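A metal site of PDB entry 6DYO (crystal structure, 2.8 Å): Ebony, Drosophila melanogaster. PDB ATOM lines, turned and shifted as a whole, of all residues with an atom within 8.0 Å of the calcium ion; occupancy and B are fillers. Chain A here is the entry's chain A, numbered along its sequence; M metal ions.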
ATOM      1  N   PHE A  79      21.560 -15.682  -0.062  1.00  0.00           N
ATOM      2  CA  PHE A  79      20.568 -14.649   0.170  1.00  0.00           C
ATOM      3  C   PHE A  79      20.563 -13.689  -1.011  1.00  0.00           C
ATOM      4  O   PHE A  79      21.543 -13.567  -1.746  1.00  0.00           O
ATOM      5  CB  PHE A  79      20.853 -13.853   1.450  1.00  0.00           C
ATOM      6  CG  PHE A  79      20.280 -14.467   2.693  1.00  0.00           C
ATOM      7  CD1 PHE A  79      18.930 -14.768   2.780  1.00  0.00           C
ATOM      8  CD2 PHE A  79      21.087 -14.717   3.786  1.00  0.00           C
ATOM      9  CE1 PHE A  79      18.410 -15.324   3.930  1.00  0.00           C
ATOM     10  CE2 PHE A  79      20.581 -15.272   4.938  1.00  0.00           C
ATOM     11  CZ  PHE A  79      19.235 -15.576   5.009  1.00  0.00           C
ATOM     12  N   ASP A  80      19.435 -12.997  -1.174  1.00  0.00           N
ATOM     13  CA  ASP A  80      19.415 -11.811  -2.018  1.00  0.00           C
ATOM     14  C   ASP A  80      20.280 -10.748  -1.364  1.00  0.00           C
ATOM     15  O   ASP A  80      20.025 -10.342  -0.225  1.00  0.00           O
ATOM     16  CB  ASP A  80      17.982 -11.318  -2.201  1.00  0.00           C
ATOM     17  CG  ASP A  80      17.848 -10.225  -3.264  1.00  0.00           C
ATOM     18  OD1 ASP A  80      18.840  -9.513  -3.532  1.00  0.00           O
ATOM     19  OD2 ASP A  80      16.745 -10.082  -3.828  1.00  0.00           O
ATOM     20  N   ALA A  81      21.324 -10.302  -2.079  1.00  0.00           N
ATOM     21  CA  ALA A  81      22.280  -9.377  -1.466  1.00  0.00           C
ATOM     22  C   ALA A  81      21.625  -8.067  -1.073  1.00  0.00           C
ATOM     23  O   ALA A  81      22.082  -7.407  -0.120  1.00  0.00           O
ATOM     24  CB  ALA A  81      23.450  -9.120  -2.421  1.00  0.00           C
ATOM     25  N   ARG A  82      20.560  -7.664  -1.760  1.00  0.00           N
ATOM     26  CA  ARG A  82      19.824  -6.452  -1.423  1.00  0.00           C
ATOM     27  C   ARG A  82      18.583  -6.750  -0.586  1.00  0.00           C
ATOM     28  O   ARG A  82      17.673  -5.928  -0.501  1.00  0.00           O
ATOM     29  CB  ARG A  82      19.441  -5.695  -2.697  1.00  0.00           C
ATOM     30  CG  ARG A  82      20.617  -5.396  -3.611  1.00  0.00           C
ATOM     31  CD  ARG A  82      20.387  -4.132  -4.422  1.00  0.00           C
ATOM     32  NE  ARG A  82      21.528  -3.800  -5.268  1.00  0.00           N
ATOM     33  CZ  ARG A  82      22.661  -3.247  -4.836  1.00  0.00           C
ATOM     34  NH1 ARG A  82      23.638  -2.978  -5.682  1.00  0.00           N
ATOM     35  NH2 ARG A  82      22.806  -2.957  -3.549  1.00  0.00           N
ATOM     36  N   ASN A  83      18.528  -7.935   0.048  1.00  0.00           N
ATOM     37  CA  ASN A  83      17.404  -8.314   0.885  1.00  0.00           C
ATOM     38  C   ASN A  83      17.836  -9.254   2.003  1.00  0.00           C
ATOM     39  O   ASN A  83      17.049 -10.114   2.433  1.00  0.00           O
ATOM     40  CB  ASN A  83      16.293  -8.968   0.043  1.00  0.00           C
ATOM     41  CG  ASN A  83      14.948  -8.971   0.742  1.00  0.00           C
ATOM     42  OD1 ASN A  83      14.737  -8.245   1.713  1.00  0.00           O
ATOM     43  ND2 ASN A  83      14.029  -9.787   0.246  1.00  0.00           N
ATOM     44  N   ARG A 108      29.186  -3.128  -3.788  1.00  0.00           N
ATOM     45  CA  ARG A 108      27.839  -3.621  -4.050  1.00  0.00           C
ATOM     46  C   ARG A 108      26.881  -2.488  -4.417  1.00  0.00           C
ATOM     47  O   ARG A 108      26.020  -2.655  -5.289  1.00  0.00           O
ATOM     48  CB  ARG A 108      27.322  -4.394  -2.839  1.00  0.00           C
ATOM     49  CG  ARG A 108      25.854  -4.786  -2.918  1.00  0.00           C
ATOM     50  CD  ARG A 108      25.346  -5.239  -1.558  1.00  0.00           C
ATOM     51  NE  ARG A 108      25.364  -4.152  -0.584  1.00  0.00           N
ATOM     52  CZ  ARG A 108      26.125  -4.142   0.511  1.00  0.00           C
ATOM     53  NH1 ARG A 108      26.931  -5.156   0.773  1.00  0.00           N
ATOM     54  NH2 ARG A 108      26.073  -3.108   1.340  1.00  0.00           N
ATOM     55  N   PRO A 113      24.557  -4.131 -10.008  1.00  0.00           N
ATOM     56  CA  PRO A 113      23.245  -3.620 -10.404  1.00  0.00           C
ATOM     57  C   PRO A 113      22.346  -3.315  -9.217  1.00  0.00           C
ATOM     58  O   PRO A 113      22.354  -4.007  -8.207  1.00  0.00           O
ATOM     59  CB  PRO A 113      22.670  -4.771 -11.251  1.00  0.00           C
ATOM     60  CG  PRO A 113      23.860  -5.481 -11.766  1.00  0.00           C
ATOM     61  CD  PRO A 113      24.867  -5.412 -10.667  1.00  0.00           C
ATOM     62  N   LYS A 114      21.560  -2.247  -9.371  1.00  0.00           N
ATOM     63  CA  LYS A 114      20.599  -1.840  -8.361  1.00  0.00           C
ATOM     64  C   LYS A 114      19.321  -2.681  -8.481  1.00  0.00           C
ATOM     65  O   LYS A 114      19.074  -3.345  -9.490  1.00  0.00           O
ATOM     66  CB  LYS A 114      20.252  -0.360  -8.508  1.00  0.00           C
ATOM     67  CG  LYS A 114      21.459   0.552  -8.638  1.00  0.00           C
ATOM     68  CD  LYS A 114      21.951   1.046  -7.285  1.00  0.00           C
ATOM     69  CE  LYS A 114      23.380   1.547  -7.360  1.00  0.00           C
ATOM     70  NZ  LYS A 114      24.372   0.431  -7.418  1.00  0.00           N
ATOM     71  N   GLY A 115      18.511  -2.643  -7.431  1.00  0.00           N
ATOM     72  CA  GLY A 115      17.262  -3.352  -7.412  1.00  0.00           C
ATOM     73  C   GLY A 115      17.414  -4.769  -6.869  1.00  0.00           C
ATOM     74  O   GLY A 115      18.491  -5.339  -6.811  1.00  0.00           O
ATOM     75  N   LEU A 116      16.273  -5.336  -6.467  1.00  0.00           N
ATOM     76  CA  LEU A 116      16.249  -6.679  -5.920  1.00  0.00           C
ATOM     77  C   LEU A 116      16.274  -7.714  -7.043  1.00  0.00           C
ATOM     78  O   LEU A 116      16.060  -7.408  -8.216  1.00  0.00           O
ATOM     79  CB  LEU A 116      15.032  -6.880  -5.034  1.00  0.00           C
ATOM     80  CG  LEU A 116      14.672  -5.689  -4.126  1.00  0.00           C
ATOM     81  CD1 LEU A 116      13.391  -5.958  -3.368  1.00  0.00           C
ATOM     82  CD2 LEU A 116      15.820  -5.382  -3.168  1.00  0.00           C
ATOM     83  N   ASN A 117      16.540  -8.970  -6.660  1.00  0.00           N
ATOM     84  CA  ASN A 117      16.688 -10.084  -7.598  1.00  0.00           C
ATOM     85  C   ASN A 117      17.766  -9.786  -8.641  1.00  0.00           C
ATOM     86  O   ASN A 117      17.636 -10.120  -9.820  1.00  0.00           O
ATOM     87  CB  ASN A 117      15.365 -10.437  -8.269  1.00  0.00           C
ATOM     88  CG  ASN A 117      15.291 -11.894  -8.698  1.00  0.00           C
ATOM     89  OD1 ASN A 117      16.249 -12.441  -9.252  1.00  0.00           O
ATOM     90  ND2 ASN A 117      14.155 -12.530  -8.437  1.00  0.00           N
ATOM     91  N   GLN A 118      18.853  -9.149  -8.198  1.00  0.00           N
ATOM     92  CA  GLN A 118      19.992  -8.866  -9.062  1.00  0.00           C
ATOM     93  C   GLN A 118      21.262  -9.540  -8.574  1.00  0.00           C
ATOM     94  O   GLN A 118      21.953 -10.196  -9.375  1.00  0.00           O
ATOM     95  CB  GLN A 118      20.223  -7.345  -9.168  1.00  0.00           C
ATOM     96  CG  GLN A 118      19.069  -6.567  -9.776  1.00  0.00           C
ATOM     97  CD  GLN A 118      19.024  -6.668 -11.281  1.00  0.00           C
ATOM     98  OE1 GLN A 118      19.818  -7.388 -11.893  1.00  0.00           O
ATOM     99  NE2 GLN A 118      18.093  -5.940 -11.900  1.00  0.00           N
ATOM    100  N   ILE A 119      21.578  -9.423  -7.293  1.00  0.00           N
ATOM    101  CA  ILE A 119      22.834  -9.912  -6.750  1.00  0.00           C
ATOM    102  C   ILE A 119      22.536 -11.084  -5.831  1.00  0.00           C
ATOM    103  O   ILE A 119      21.967 -10.910  -4.749  1.00  0.00           O
ATOM    104  CB  ILE A 119      23.594  -8.808  -6.011  1.00  0.00           C
ATOM    105  CG1 ILE A 119      23.551  -7.504  -6.804  1.00  0.00           C
ATOM    106  CG2 ILE A 119      25.019  -9.223  -5.746  1.00  0.00           C
ATOM    107  CD1 ILE A 119      24.070  -6.303  -6.046  1.00  0.00           C
ATOM    108  N   LEU A 120      22.923 -12.286  -6.258  1.00  0.00           N
ATOM    109  CA  LEU A 120      22.823 -13.485  -5.429  1.00  0.00           C
ATOM    110  C   LEU A 120      24.100 -13.619  -4.616  1.00  0.00           C
ATOM    111  O   LEU A 120      25.162 -13.951  -5.148  1.00  0.00           O
ATOM    112  CB  LEU A 120      22.598 -14.726  -6.300  1.00  0.00           C
ATOM    113  CG  LEU A 120      22.308 -16.029  -5.560  1.00  0.00           C
ATOM    114  CD1 LEU A 120      20.943 -15.974  -4.886  1.00  0.00           C
ATOM    115  CD2 LEU A 120      22.397 -17.219  -6.505  1.00  0.00           C
ATOM    116  N   HIS A 121      24.010 -13.336  -3.318  1.00  0.00           N
ATOM    117  CA  HIS A 121      25.171 -13.303  -2.442  1.00  0.00           C
ATOM    118  C   HIS A 121      25.412 -14.702  -1.887  1.00  0.00           C
ATOM    119  O   HIS A 121      24.584 -15.235  -1.145  1.00  0.00           O
ATOM    120  CB  HIS A 121      24.980 -12.304  -1.301  1.00  0.00           C
ATOM    121  CG  HIS A 121      26.121 -12.250  -0.343  1.00  0.00           C
ATOM    122  ND1 HIS A 121      25.962 -11.896   0.980  1.00  0.00           N
ATOM    123  CD2 HIS A 121      27.445 -12.507  -0.504  1.00  0.00           C
ATOM    124  CE1 HIS A 121      27.137 -11.930   1.596  1.00  0.00           C
ATOM    125  NE2 HIS A 121      28.052 -12.306   0.713  1.00  0.00           N
ATOM    126  N   PHE A 156      18.608 -14.184 -11.603  1.00  0.00           N
ATOM    127  CA  PHE A 156      19.522 -13.239 -10.981  1.00  0.00           C
ATOM    128  C   PHE A 156      20.528 -12.715 -12.007  1.00  0.00           C
ATOM    129  O   PHE A 156      20.765 -13.346 -13.045  1.00  0.00           O
ATOM    130  CB  PHE A 156      20.262 -13.875  -9.802  1.00  0.00           C
ATOM    131  CG  PHE A 156      19.515 -13.779  -8.500  1.00  0.00           C
ATOM    132  CD1 PHE A 156      18.564 -14.722  -8.163  1.00  0.00           C
ATOM    133  CD2 PHE A 156      19.775 -12.752  -7.615  1.00  0.00           C
ATOM    134  CE1 PHE A 156      17.884 -14.639  -6.964  1.00  0.00           C
ATOM    135  CE2 PHE A 156      19.101 -12.656  -6.418  1.00  0.00           C
ATOM    136  CZ  PHE A 156      18.146 -13.607  -6.092  1.00  0.00           C
ATOM    137  N   ALA A 157      21.106 -11.553 -11.715  1.00  0.00           N
ATOM    138  CA  ALA A 157      22.087 -10.977 -12.625  1.00  0.00           C
ATOM    139  C   ALA A 157      23.451 -11.630 -12.468  1.00  0.00           C
ATOM    140  O   ALA A 157      24.112 -11.931 -13.464  1.00  0.00           O
ATOM    141  CB  ALA A 157      22.188  -9.470 -12.410  1.00  0.00           C
ATOM    142  N   GLY A 158      23.889 -11.859 -11.234  1.00  0.00           N
ATOM    143  CA  GLY A 158      25.166 -12.498 -11.022  1.00  0.00           C
ATOM    144  C   GLY A 158      25.291 -13.059  -9.624  1.00  0.00           C
ATOM    145  O   GLY A 158      24.372 -12.954  -8.808  1.00  0.00           O
HETATM  146 CA    CA M   1      19.516  -8.124  -5.790  1.00  0.00          CA
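The backbone NH (N) of Ala 157 lies within hydrogen-bond range of the backbone carbonyl oxygen (O) of Gln 118 (2.8 Å).
O of Gln 118 sits at hydrogen-bond distance from N of Gly 158 (3.2 Å).
The backbone carbonyl oxygen (O) of Ile 119 sits at hydrogen-bond distance from the backbone NH (N) of Ala 81, 2.8 Å away.
The backbone NH (N) of Arg 82 lies close to the side-chain carboxylate (OD1) of Asp 80, at 3.1 Å.
NH1 of Arg 82 sits at hydrogen-bond distance from O of Arg 108.
The side-chain carboxylate (OD2) of Asp 80 is in hydrogen-bond range of the backbone NH (N) of Asn 117 (3.0 Å).
NH1 of Arg 82 sits at hydrogen-bond distance from O of Pro 113, at 3.0 Å.
Residues that only touch the calcium ion: Arg 82 (3.7 Å), Leu 116 (3.5 Å) and Asn 117 (3.2 Å).
The nearest printed residue that does not touch the calcium ion is Phe 156 (4.6 Å).
The calcium ion is bound by the backbone nitrogen of Gln 118, the side-chain carboxylate of Asp 80 and the backbone nitrogen of Ile 119.
Slightly farther from the calcium ion lies O of Gly 115 (3.1 Å).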
